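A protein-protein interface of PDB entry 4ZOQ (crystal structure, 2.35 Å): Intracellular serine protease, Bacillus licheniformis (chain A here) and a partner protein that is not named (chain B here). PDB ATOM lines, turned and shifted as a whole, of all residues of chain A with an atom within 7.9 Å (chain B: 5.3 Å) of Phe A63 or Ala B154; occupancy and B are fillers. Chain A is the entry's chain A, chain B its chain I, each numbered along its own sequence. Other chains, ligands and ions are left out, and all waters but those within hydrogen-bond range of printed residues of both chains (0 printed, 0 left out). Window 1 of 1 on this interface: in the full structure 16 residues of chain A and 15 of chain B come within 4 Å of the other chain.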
ATOM      1  N   GLN A  31      -9.047  21.603  12.500  1.00  0.00           N
ATOM      2  CA  GLN A  31     -10.340  21.417  13.160  1.00  0.00           C
ATOM      3  C   GLN A  31     -10.888  22.710  13.784  1.00  0.00           C
ATOM      4  O   GLN A  31     -10.273  23.769  13.673  1.00  0.00           O
ATOM      5  CB  GLN A  31     -10.266  20.326  14.222  1.00  0.00           C
ATOM      6  CG  GLN A  31      -9.572  19.089  13.740  1.00  0.00           C
ATOM      7  CD  GLN A  31      -9.564  18.014  14.777  1.00  0.00           C
ATOM      8  OE1 GLN A  31      -9.711  16.836  14.460  1.00  0.00           O
ATOM      9  NE2 GLN A  31      -9.422  18.406  16.029  1.00  0.00           N
ATOM     10  N   TYR A  32     -12.059  22.616  14.415  1.00  0.00           N
ATOM     11  CA  TYR A  32     -12.729  23.788  14.973  1.00  0.00           C
ATOM     12  C   TYR A  32     -13.233  23.531  16.391  1.00  0.00           C
ATOM     13  O   TYR A  32     -13.660  22.417  16.731  1.00  0.00           O
ATOM     14  CB  TYR A  32     -13.901  24.235  14.085  1.00  0.00           C
ATOM     15  CG  TYR A  32     -13.490  24.775  12.735  1.00  0.00           C
ATOM     16  CD1 TYR A  32     -13.366  23.931  11.629  1.00  0.00           C
ATOM     17  CD2 TYR A  32     -13.223  26.128  12.562  1.00  0.00           C
ATOM     18  CE1 TYR A  32     -12.973  24.430  10.389  1.00  0.00           C
ATOM     19  CE2 TYR A  32     -12.839  26.633  11.319  1.00  0.00           C
ATOM     20  CZ  TYR A  32     -12.713  25.780  10.246  1.00  0.00           C
ATOM     21  OH  TYR A  32     -12.336  26.290   9.028  1.00  0.00           O
ATOM     22  N   LEU A  33     -13.196  24.576  17.210  1.00  0.00           N
ATOM     23  CA  LEU A  33     -13.563  24.469  18.609  1.00  0.00           C
ATOM     24  C   LEU A  33     -14.533  25.553  19.056  1.00  0.00           C
ATOM     25  O   LEU A  33     -14.377  26.725  18.714  1.00  0.00           O
ATOM     26  CB  LEU A  33     -12.312  24.551  19.501  1.00  0.00           C
ATOM     27  CG  LEU A  33     -11.428  23.352  19.826  1.00  0.00           C
ATOM     28  CD1 LEU A  33     -10.075  23.839  20.273  1.00  0.00           C
ATOM     29  CD2 LEU A  33     -12.059  22.555  20.937  1.00  0.00           C
ATOM     30  N   LEU A  34     -15.496  25.164  19.877  1.00  0.00           N
ATOM     31  CA  LEU A  34     -16.385  26.119  20.478  1.00  0.00           C
ATOM     32  C   LEU A  34     -16.263  26.005  22.000  1.00  0.00           C
ATOM     33  O   LEU A  34     -16.599  24.974  22.573  1.00  0.00           O
ATOM     34  CB  LEU A  34     -17.829  25.906  20.010  1.00  0.00           C
ATOM     35  CG  LEU A  34     -18.736  26.989  20.582  1.00  0.00           C
ATOM     36  CD1 LEU A  34     -18.280  28.366  20.088  1.00  0.00           C
ATOM     37  CD2 LEU A  34     -20.193  26.741  20.209  1.00  0.00           C
ATOM     38  N   LEU A  35     -15.710  27.027  22.651  1.00  0.00           N
ATOM     39  CA  LEU A  35     -15.624  27.034  24.114  1.00  0.00           C
ATOM     40  C   LEU A  35     -17.008  27.178  24.742  1.00  0.00           C
ATOM     41  O   LEU A  35     -17.877  27.857  24.207  1.00  0.00           O
ATOM     42  CB  LEU A  35     -14.715  28.179  24.604  1.00  0.00           C
ATOM     43  CG  LEU A  35     -13.292  28.327  24.066  1.00  0.00           C
ATOM     44  CD1 LEU A  35     -12.762  29.714  24.336  1.00  0.00           C
ATOM     45  CD2 LEU A  35     -12.379  27.310  24.715  1.00  0.00           C
ATOM     46  N   HIS A  37     -17.246  28.712  27.461  1.00  0.00           N
ATOM     47  CA  HIS A  37     -17.136  30.051  28.008  1.00  0.00           C
ATOM     48  C   HIS A  37     -16.035  30.810  27.326  1.00  0.00           C
ATOM     49  O   HIS A  37     -14.907  30.340  27.236  1.00  0.00           O
ATOM     50  CB  HIS A  37     -16.848  29.992  29.511  1.00  0.00           C
ATOM     51  CG  HIS A  37     -17.843  29.187  30.287  1.00  0.00           C
ATOM     52  ND1 HIS A  37     -17.740  27.818  30.428  1.00  0.00           N
ATOM     53  CD2 HIS A  37     -18.956  29.553  30.965  1.00  0.00           C
ATOM     54  CE1 HIS A  37     -18.745  27.376  31.163  1.00  0.00           C
ATOM     55  NE2 HIS A  37     -19.498  28.409  31.500  1.00  0.00           N
ATOM     56  N   VAL A  38     -16.370  31.999  26.849  1.00  0.00           N
ATOM     57  CA  VAL A  38     -15.448  32.744  26.021  1.00  0.00           C
ATOM     58  C   VAL A  38     -14.315  33.303  26.878  1.00  0.00           C
ATOM     59  O   VAL A  38     -13.292  33.714  26.351  1.00  0.00           O
ATOM     60  CB  VAL A  38     -16.174  33.850  25.215  1.00  0.00           C
ATOM     61  CG1 VAL A  38     -17.416  33.282  24.517  1.00  0.00           C
ATOM     62  CG2 VAL A  38     -16.458  35.078  26.072  1.00  0.00           C
ATOM     63  N   LYS A  41     -10.626  31.731  26.519  1.00  0.00           N
ATOM     64  CA  LYS A  41      -9.854  31.883  25.298  1.00  0.00           C
ATOM     65  C   LYS A  41      -8.354  31.808  25.614  1.00  0.00           C
ATOM     66  O   LYS A  41      -7.570  31.180  24.892  1.00  0.00           O
ATOM     67  CB  LYS A  41     -10.201  33.196  24.613  1.00  0.00           C
ATOM     68  CG  LYS A  41      -9.242  33.642  23.518  1.00  0.00           C
ATOM     69  CD  LYS A  41      -9.320  35.149  23.346  1.00  0.00           C
ATOM     70  CE  LYS A  41      -8.421  35.668  22.234  1.00  0.00           C
ATOM     71  NZ  LYS A  41      -7.079  36.109  22.695  1.00  0.00           N
ATOM     72  N   LEU A  44      -6.978  28.471  26.212  1.00  0.00           N
ATOM     73  CA  LEU A  44      -6.975  27.789  24.930  1.00  0.00           C
ATOM     74  C   LEU A  44      -5.722  28.087  24.148  1.00  0.00           C
ATOM     75  O   LEU A  44      -5.120  27.188  23.563  1.00  0.00           O
ATOM     76  CB  LEU A  44      -8.198  28.234  24.123  1.00  0.00           C
ATOM     77  CG  LEU A  44      -8.285  27.875  22.641  1.00  0.00           C
ATOM     78  CD1 LEU A  44      -8.353  26.393  22.408  1.00  0.00           C
ATOM     79  CD2 LEU A  44      -9.459  28.575  22.012  1.00  0.00           C
ATOM     80  N   ALA A  55      -4.106  28.145  16.824  1.00  0.00           N
ATOM     81  CA  ALA A  55      -5.494  28.359  17.162  1.00  0.00           C
ATOM     82  C   ALA A  55      -5.890  29.807  16.925  1.00  0.00           C
ATOM     83  O   ALA A  55      -5.374  30.742  17.557  1.00  0.00           O
ATOM     84  CB  ALA A  55      -5.736  27.986  18.610  1.00  0.00           C
ATOM     85  N   ASP A  56      -6.836  29.975  16.011  1.00  0.00           N
ATOM     86  CA  ASP A  56      -7.332  31.286  15.640  1.00  0.00           C
ATOM     87  C   ASP A  56      -8.705  31.419  16.243  1.00  0.00           C
ATOM     88  O   ASP A  56      -9.625  30.724  15.843  1.00  0.00           O
ATOM     89  CB  ASP A  56      -7.393  31.432  14.127  1.00  0.00           C
ATOM     90  CG  ASP A  56      -7.749  32.838  13.685  1.00  0.00           C
ATOM     91  OD1 ASP A  56      -8.151  33.656  14.544  1.00  0.00           O
ATOM     92  OD2 ASP A  56      -7.687  33.104  12.460  1.00  0.00           O
ATOM     93  N   VAL A  57      -8.841  32.310  17.214  1.00  0.00           N
ATOM     94  CA  VAL A  57     -10.071  32.407  17.974  1.00  0.00           C
ATOM     95  C   VAL A  57     -10.790  33.680  17.644  1.00  0.00           C
ATOM     96  O   VAL A  57     -10.164  34.740  17.529  1.00  0.00           O
ATOM     97  CB  VAL A  57      -9.825  32.375  19.478  1.00  0.00           C
ATOM     98  CG1 VAL A  57     -11.134  32.144  20.214  1.00  0.00           C
ATOM     99  CG2 VAL A  57      -8.838  31.296  19.804  1.00  0.00           C
ATOM    100  N   ILE A  58     -12.099  33.547  17.427  1.00  0.00           N
ATOM    101  CA  ILE A  58     -13.019  34.672  17.374  1.00  0.00           C
ATOM    102  C   ILE A  58     -13.491  34.920  18.789  1.00  0.00           C
ATOM    103  O   ILE A  58     -14.404  34.248  19.277  1.00  0.00           O
ATOM    104  CB  ILE A  58     -14.225  34.415  16.406  1.00  0.00           C
ATOM    105  CG1 ILE A  58     -13.731  34.021  15.018  1.00  0.00           C
ATOM    106  CG2 ILE A  58     -15.116  35.659  16.276  1.00  0.00           C
ATOM    107  CD1 ILE A  58     -14.807  33.435  14.132  1.00  0.00           C
ATOM    108  N   GLU A  59     -12.847  35.869  19.460  1.00  0.00           N
ATOM    109  CA  GLU A  59     -12.977  36.029  20.913  1.00  0.00           C
ATOM    110  C   GLU A  59     -14.400  36.189  21.439  1.00  0.00           C
ATOM    111  O   GLU A  59     -14.768  35.609  22.453  1.00  0.00           O
ATOM    112  CB  GLU A  59     -12.183  37.259  21.352  1.00  0.00           C
ATOM    113  CG  GLU A  59     -12.306  37.576  22.833  1.00  0.00           C
ATOM    114  CD  GLU A  59     -11.374  38.699  23.252  1.00  0.00           C
ATOM    115  OE1 GLU A  59     -10.494  39.071  22.440  1.00  0.00           O
ATOM    116  OE2 GLU A  59     -11.560  39.250  24.362  1.00  0.00           O
ATOM    117  N   GLU A  60     -15.198  36.988  20.748  1.00  0.00           N
ATOM    118  CA  GLU A  60     -16.517  37.334  21.251  1.00  0.00           C
ATOM    119  C   GLU A  60     -17.466  36.152  21.279  1.00  0.00           C
ATOM    120  O   GLU A  60     -18.433  36.143  22.022  1.00  0.00           O
ATOM    121  CB  GLU A  60     -17.110  38.477  20.440  1.00  0.00           C
ATOM    122  CG  GLU A  60     -16.373  39.806  20.616  1.00  0.00           C
ATOM    123  CD  GLU A  60     -15.167  39.923  19.714  1.00  0.00           C
ATOM    124  OE1 GLU A  60     -14.727  38.898  19.154  1.00  0.00           O
ATOM    125  OE2 GLU A  60     -14.660  41.051  19.540  1.00  0.00           O
ATOM    126  N   ILE A  61     -17.201  35.157  20.459  1.00  0.00           N
ATOM    127  CA  ILE A  61     -18.080  33.992  20.394  1.00  0.00           C
ATOM    128  C   ILE A  61     -17.358  32.706  20.823  1.00  0.00           C
ATOM    129  O   ILE A  61     -17.957  31.627  20.832  1.00  0.00           O
ATOM    130  CB  ILE A  61     -18.724  33.840  18.978  1.00  0.00           C
ATOM    131  CG1 ILE A  61     -17.676  33.694  17.885  1.00  0.00           C
ATOM    132  CG2 ILE A  61     -19.666  35.031  18.679  1.00  0.00           C
ATOM    133  CD1 ILE A  61     -18.294  33.325  16.555  1.00  0.00           C
ATOM    134  N   GLY A  62     -16.052  32.803  21.078  1.00  0.00           N
ATOM    135  CA  GLY A  62     -15.316  31.691  21.654  1.00  0.00           C
ATOM    136  C   GLY A  62     -15.215  30.501  20.727  1.00  0.00           C
ATOM    137  O   GLY A  62     -15.297  29.354  21.157  1.00  0.00           O
ATOM    138  N   PHE A  63     -15.025  30.797  19.451  1.00  0.00           N
ATOM    139  CA  PHE A  63     -14.998  29.806  18.393  1.00  0.00           C
ATOM    140  C   PHE A  63     -13.676  29.890  17.645  1.00  0.00           C
ATOM    141  O   PHE A  63     -13.292  30.950  17.138  1.00  0.00           O
ATOM    142  CB  PHE A  63     -16.211  30.025  17.466  1.00  0.00           C
ATOM    143  CG  PHE A  63     -16.415  28.944  16.437  1.00  0.00           C
ATOM    144  CD1 PHE A  63     -16.649  27.633  16.810  1.00  0.00           C
ATOM    145  CD2 PHE A  63     -16.414  29.260  15.081  1.00  0.00           C
ATOM    146  CE1 PHE A  63     -16.843  26.648  15.858  1.00  0.00           C
ATOM    147  CE2 PHE A  63     -16.615  28.275  14.125  1.00  0.00           C
ATOM    148  CZ  PHE A  63     -16.830  26.965  14.520  1.00  0.00           C
ATOM    149  N   ALA A  64     -12.986  28.765  17.551  1.00  0.00           N
ATOM    150  CA  ALA A  64     -11.614  28.804  17.086  1.00  0.00           C
ATOM    151  C   ALA A  64     -11.323  27.813  15.977  1.00  0.00           C
ATOM    152  O   ALA A  64     -11.864  26.716  15.958  1.00  0.00           O
ATOM    153  CB  ALA A  64     -10.665  28.562  18.258  1.00  0.00           C
ATOM    154  N   LYS A  65     -10.434  28.190  15.075  1.00  0.00           N
ATOM    155  CA  LYS A  65      -9.965  27.232  14.094  1.00  0.00           C
ATOM    156  C   LYS A  65      -8.550  26.825  14.503  1.00  0.00           C
ATOM    157  O   LYS A  65      -7.675  27.663  14.722  1.00  0.00           O
ATOM    158  CB  LYS A  65      -9.998  27.807  12.668  1.00  0.00           C
ATOM    159  CG  LYS A  65      -9.104  27.067  11.666  1.00  0.00           C
ATOM    160  CD  LYS A  65      -9.139  27.693  10.266  1.00  0.00           C
ATOM    161  CE  LYS A  65      -8.712  29.139  10.274  1.00  0.00           C
ATOM    162  NZ  LYS A  65      -7.303  29.342  10.721  1.00  0.00           N
ATOM    163  N   VAL A  66      -8.343  25.530  14.663  1.00  0.00           N
ATOM    164  CA  VAL A  66      -7.051  25.048  15.113  1.00  0.00           C
ATOM    165  C   VAL A  66      -6.406  24.292  13.959  1.00  0.00           C
ATOM    166  O   VAL A  66      -7.010  23.420  13.338  1.00  0.00           O
ATOM    167  CB  VAL A  66      -7.155  24.156  16.379  1.00  0.00           C
ATOM    168  CG1 VAL A  66      -7.656  24.971  17.556  1.00  0.00           C
ATOM    169  CG2 VAL A  66      -8.072  22.989  16.140  1.00  0.00           C
ATOM    170  N   ASP A  87     -16.405  21.971  22.624  1.00  0.00           N
ATOM    171  CA  ASP A  87     -16.836  20.922  21.691  1.00  0.00           C
ATOM    172  C   ASP A  87     -15.990  21.082  20.433  1.00  0.00           C
ATOM    173  O   ASP A  87     -15.627  22.201  20.077  1.00  0.00           O
ATOM    174  CB  ASP A  87     -18.343  21.012  21.371  1.00  0.00           C
ATOM    175  CG  ASP A  87     -19.218  21.037  22.620  1.00  0.00           C
ATOM    176  OD1 ASP A  87     -18.785  20.533  23.676  1.00  0.00           O
ATOM    177  OD2 ASP A  87     -20.336  21.585  22.565  1.00  0.00           O
ATOM    178  N   VAL A  88     -15.669  19.973  19.770  1.00  0.00           N
ATOM    179  CA  VAL A  88     -14.717  19.987  18.655  1.00  0.00           C
ATOM    180  C   VAL A  88     -15.351  19.546  17.338  1.00  0.00           C
ATOM    181  O   VAL A  88     -16.134  18.607  17.314  1.00  0.00           O
ATOM    182  CB  VAL A  88     -13.521  19.061  18.970  1.00  0.00           C
ATOM    183  CG1 VAL A  88     -12.400  19.236  17.974  1.00  0.00           C
ATOM    184  CG2 VAL A  88     -13.036  19.306  20.384  1.00  0.00           C
ATOM    185  N   ILE A  89     -14.967  20.168  16.228  1.00  0.00           N
ATOM    186  CA  ILE A  89     -15.515  19.754  14.948  1.00  0.00           C
ATOM    187  C   ILE A  89     -14.413  19.316  14.002  1.00  0.00           C
ATOM    188  O   ILE A  89     -13.380  19.964  13.897  1.00  0.00           O
ATOM    189  CB  ILE A  89     -16.324  20.910  14.261  1.00  0.00           C
ATOM    190  CG1 ILE A  89     -17.592  21.238  15.033  1.00  0.00           C
ATOM    191  CG2 ILE A  89     -16.705  20.557  12.823  1.00  0.00           C
ATOM    192  CD1 ILE A  89     -18.231  22.547  14.578  1.00  0.00           C
ATOM    193  N   TYR B 117     -16.936  29.648   9.190  1.00  0.00           N
ATOM    194  CA  TYR B 117     -16.072  30.253  10.195  1.00  0.00           C
ATOM    195  C   TYR B 117     -15.716  31.679   9.794  1.00  0.00           C
ATOM    196  O   TYR B 117     -15.785  32.602  10.608  1.00  0.00           O
ATOM    197  CB  TYR B 117     -14.795  29.422  10.377  1.00  0.00           C
ATOM    198  CG  TYR B 117     -13.782  30.032  11.319  1.00  0.00           C
ATOM    199  CD1 TYR B 117     -13.909  29.874  12.691  1.00  0.00           C
ATOM    200  CD2 TYR B 117     -12.724  30.810  10.840  1.00  0.00           C
ATOM    201  CE1 TYR B 117     -12.999  30.434  13.561  1.00  0.00           C
ATOM    202  CE2 TYR B 117     -11.798  31.382  11.714  1.00  0.00           C
ATOM    203  CZ  TYR B 117     -11.951  31.189  13.075  1.00  0.00           C
ATOM    204  OH  TYR B 117     -11.065  31.744  13.976  1.00  0.00           O
ATOM    205  N   MET B 120     -18.665  34.115  10.252  1.00  0.00           N
ATOM    206  CA  MET B 120     -18.820  34.514  11.651  1.00  0.00           C
ATOM    207  C   MET B 120     -17.783  35.569  12.036  1.00  0.00           C
ATOM    208  O   MET B 120     -18.114  36.572  12.674  1.00  0.00           O
ATOM    209  CB  MET B 120     -18.679  33.306  12.582  1.00  0.00           C
ATOM    210  CG  MET B 120     -19.651  32.205  12.304  1.00  0.00           C
ATOM    211  SD  MET B 120     -19.659  30.925  13.589  1.00  0.00           S
ATOM    212  CE  MET B 120     -19.952  29.482  12.557  1.00  0.00           C
ATOM    213  N   LYS B 149     -24.794  20.831  14.993  1.00  0.00           N
ATOM    214  CA  LYS B 149     -25.379  21.644  16.042  1.00  0.00           C
ATOM    215  C   LYS B 149     -24.376  22.588  16.690  1.00  0.00           C
ATOM    216  O   LYS B 149     -24.746  23.681  17.134  1.00  0.00           O
ATOM    217  CB  LYS B 149     -26.001  20.760  17.101  1.00  0.00           C
ATOM    218  CG  LYS B 149     -26.960  19.754  16.540  1.00  0.00           C
ATOM    219  CD  LYS B 149     -27.748  19.115  17.659  1.00  0.00           C
ATOM    220  CE  LYS B 149     -28.628  18.000  17.141  1.00  0.00           C
ATOM    221  NZ  LYS B 149     -29.179  17.193  18.278  1.00  0.00           N
ATOM    222  N   VAL B 150     -23.110  22.189  16.718  1.00  0.00           N
ATOM    223  CA  VAL B 150     -22.074  23.033  17.295  1.00  0.00           C
ATOM    224  C   VAL B 150     -21.831  24.234  16.384  1.00  0.00           C
ATOM    225  O   VAL B 150     -21.721  25.373  16.853  1.00  0.00           O
ATOM    226  CB  VAL B 150     -20.757  22.251  17.518  1.00  0.00           C
ATOM    227  CG1 VAL B 150     -19.625  23.215  17.806  1.00  0.00           C
ATOM    228  CG2 VAL B 150     -20.921  21.293  18.693  1.00  0.00           C
ATOM    229  N   LEU B 151     -21.759  23.972  15.081  1.00  0.00           N
ATOM    230  CA  LEU B 151     -21.628  25.037  14.087  1.00  0.00           C
ATOM    231  C   LEU B 151     -22.790  26.034  14.200  1.00  0.00           C
ATOM    232  O   LEU B 151     -22.584  27.251  14.122  1.00  0.00           O
ATOM    233  CB  LEU B 151     -21.563  24.460  12.669  1.00  0.00           C
ATOM    234  CG  LEU B 151     -21.250  25.441  11.539  1.00  0.00           C
ATOM    235  CD1 LEU B 151     -19.828  25.904  11.634  1.00  0.00           C
ATOM    236  CD2 LEU B 151     -21.525  24.823  10.161  1.00  0.00           C
ATOM    237  N   MET B 152     -24.002  25.518  14.377  1.00  0.00           N
ATOM    238  CA  MET B 152     -25.165  26.377  14.499  1.00  0.00           C
ATOM    239  C   MET B 152     -25.108  27.184  15.776  1.00  0.00           C
ATOM    240  O   MET B 152     -25.491  28.358  15.807  1.00  0.00           O
ATOM    241  CB  MET B 152     -26.460  25.560  14.427  1.00  0.00           C
ATOM    242  CG  MET B 152     -27.733  26.395  14.568  1.00  0.00           C
ATOM    243  SD  MET B 152     -29.177  25.527  13.893  1.00  0.00           S
ATOM    244  CE  MET B 152     -30.516  26.676  14.244  1.00  0.00           C
ATOM    245  N   LYS B 153     -24.640  26.535  16.836  1.00  0.00           N
ATOM    246  CA  LYS B 153     -24.507  27.160  18.147  1.00  0.00           C
ATOM    247  C   LYS B 153     -23.531  28.329  18.079  1.00  0.00           C
ATOM    248  O   LYS B 153     -23.762  29.402  18.659  1.00  0.00           O
ATOM    249  CB  LYS B 153     -24.024  26.124  19.161  1.00  0.00           C
ATOM    250  CG  LYS B 153     -23.816  26.626  20.572  1.00  0.00           C
ATOM    251  CD  LYS B 153     -23.428  25.467  21.461  1.00  0.00           C
ATOM    252  CE  LYS B 153     -23.359  25.852  22.924  1.00  0.00           C
ATOM    253  NZ  LYS B 153     -22.858  24.679  23.697  1.00  0.00           N
ATOM    254  N   ALA B 154     -22.436  28.107  17.362  1.00  0.00           N
ATOM    255  CA  ALA B 154     -21.424  29.131  17.159  1.00  0.00           C
ATOM    256  C   ALA B 154     -22.008  30.280  16.377  1.00  0.00           C
ATOM    257  O   ALA B 154     -21.818  31.463  16.693  1.00  0.00           O
ATOM    258  CB  ALA B 154     -20.215  28.547  16.406  1.00  0.00           C
ATOM    259  N   TYR B 155     -22.763  29.895  15.354  1.00  0.00           N
ATOM    260  CA  TYR B 155     -23.254  30.829  14.368  1.00  0.00           C
ATOM    261  C   TYR B 155     -24.300  31.715  15.044  1.00  0.00           C
ATOM    262  O   TYR B 155     -24.403  32.922  14.776  1.00  0.00           O
ATOM    263  CB  TYR B 155     -23.886  30.069  13.225  1.00  0.00           C
ATOM    264  CG  TYR B 155     -23.585  30.632  11.907  1.00  0.00           C
ATOM    265  CD1 TYR B 155     -23.341  29.794  10.828  1.00  0.00           C
ATOM    266  CD2 TYR B 155     -23.395  31.997  11.758  1.00  0.00           C
ATOM    267  CE1 TYR B 155     -23.038  30.309   9.598  1.00  0.00           C
ATOM    268  CE2 TYR B 155     -23.083  32.525  10.541  1.00  0.00           C
ATOM    269  CZ  TYR B 155     -22.903  31.668   9.464  1.00  0.00           C
ATOM    270  OH  TYR B 155     -22.575  32.142   8.217  1.00  0.00           O
ATOM    271  N   GLN B 156     -25.030  31.104  15.972  1.00  0.00           N
ATOM    272  CA  GLN B 156     -26.057  31.797  16.727  1.00  0.00           C
ATOM    273  C   GLN B 156     -25.432  32.834  17.666  1.00  0.00           C
ATOM    274  O   GLN B 156     -26.022  33.888  17.927  1.00  0.00           O
ATOM    275  CB  GLN B 156     -26.913  30.778  17.498  1.00  0.00           C
ATOM    276  CG  GLN B 156     -28.137  31.348  18.160  1.00  0.00           C
ATOM    277  CD  GLN B 156     -29.092  32.029  17.164  1.00  0.00           C
ATOM    278  OE1 GLN B 156     -29.756  31.367  16.352  1.00  0.00           O
ATOM    279  NE2 GLN B 156     -29.162  33.353  17.232  1.00  0.00           N
ATOM    280  N   ARG B 157     -24.219  32.569  18.136  1.00  0.00           N
ATOM    281  CA  ARG B 157     -23.575  33.511  19.039  1.00  0.00           C
ATOM    282  C   ARG B 157     -23.156  34.745  18.278  1.00  0.00           C
ATOM    283  O   ARG B 157     -23.316  35.857  18.767  1.00  0.00           O
ATOM    284  CB  ARG B 157     -22.349  32.876  19.694  1.00  0.00           C
ATOM    285  CG  ARG B 157     -22.633  31.866  20.770  1.00  0.00           C
ATOM    286  CD  ARG B 157     -21.319  31.381  21.376  1.00  0.00           C
ATOM    287  NE  ARG B 157     -21.525  30.338  22.371  1.00  0.00           N
ATOM    288  CZ  ARG B 157     -20.551  29.766  23.076  1.00  0.00           C
ATOM    289  NH1 ARG B 157     -19.285  30.110  22.873  1.00  0.00           N
ATOM    290  NH2 ARG B 157     -20.846  28.836  23.977  1.00  0.00           N
ATOM    291  N   ALA B 158     -22.700  34.552  17.047  1.00  0.00           N
ATOM    292  CA  ALA B 158     -22.378  35.668  16.167  1.00  0.00           C
ATOM    293  C   ALA B 158     -23.608  36.540  15.934  1.00  0.00           C
ATOM    294  O   ALA B 158     -23.542  37.780  16.017  1.00  0.00           O
ATOM    295  CB  ALA B 158     -21.828  35.156  14.843  1.00  0.00           C
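Tyr A32 touches Tyr B117. CG1 of Val B150 touches CB of Leu A34, at 3.9 Å. Lys B153 touches Leu A34. Arg B157 touches Leu A34 (NH1 to CD1, 3.4 Å). Tyr B117 touches Val A57 (OH to N, 3.97 Å). CB of Met B120 touches CD1 of Ile A61 (3.99 Å). Ile A61 touches Ala B154. Phe A63 touches Met B120. Phe A63 touches Ala B154 (CD1 to CB, 3.7 Å). Lys A65 touches Tyr B117.
Phe A63 touches three residues of chain B. Of the printed residues of chain A, Ala B154 touches Leu A34, Ile A61 and Phe A63. Of the printed residues of chain B, Ile A89 touches Val B150 (3.6 Å) and Leu B151 (3.8 Å). Printed residues of chain B within 4 Å of Leu A34: Val B150, Lys B153, Ala B154 and Arg B157. Of the printed residues of chain B, Ile A61 touches Met B120, Ala B154, Arg B157 and Ala B158. Tyr B155 touches none of the printed residues of chain A. Glu A60 touches none of the printed residues of chain B. The nearest residue of chain B that does not touch Phe A63 is Leu B151 (4.3 Å). The nearest printed residue of chain B that does not touch Tyr A32 is Val B150 (6.1 Å).
The backbone carbonyl oxygen (O) of Ile A61 is in hydrogen-bond range of the guanidinium group (NH1) of Arg B157, 2.9 Å away. The backbone carbonyl oxygen (O) of Leu A35 sits at hydrogen-bond distance from the guanidinium group (NH1) of Arg B157 (3.0 Å). The side-chain hydroxyl (OH) of Tyr B117 sits at hydrogen-bond distance from the backbone carbonyl oxygen (O) of Asp A56 (2.6 Å).
Of the 24 printed residues of chain A, 12 touch a printed residue of chain B. Printed residues of chain A that touch a printed residue of chain B: Tyr A32, Leu A34, Leu A35, Asp A56, Val A57, Ile A58, Ile A61, Phe A63, Ala A64, Lys A65, Asp A87 and Ile A89. Hydrophobic or aromatic side chains of chain A within 4 Å of the printed part of chain B: Tyr A32, Leu A34, Ile A58, Ile A61, Phe A63 and Ile A89. Printed residues of chain B that touch a printed residue of chain A: Tyr B117, Met B120, Val B150, Leu B151, Lys B153, Ala B154, Arg B157 and Ala B158. Among the printed residues, no Asp or Glu carboxylate lies within 4 Å of a Lys or Arg side-chain nitrogen of the other chain.
O of Asp A87 is in hydrogen-bond range of N of Leu A34, at 3.0 Å. The backbone NH of Ala A64 sits at hydrogen-bond distance from the backbone carbonyl oxygen of Leu A33 (2.7 Å). N of Ile A89 is in hydrogen-bond range of O of Tyr A32. SD of Met B120 sits close to N of Tyr B155 (3.7 Å). The backbone carbonyl oxygen (O) of Phe A63 lies within hydrogen-bond range of the backbone NH (N) of Ile A58. N of Lys A65 is in hydrogen-bond range of O of Asp A56, 2.8 Å away.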
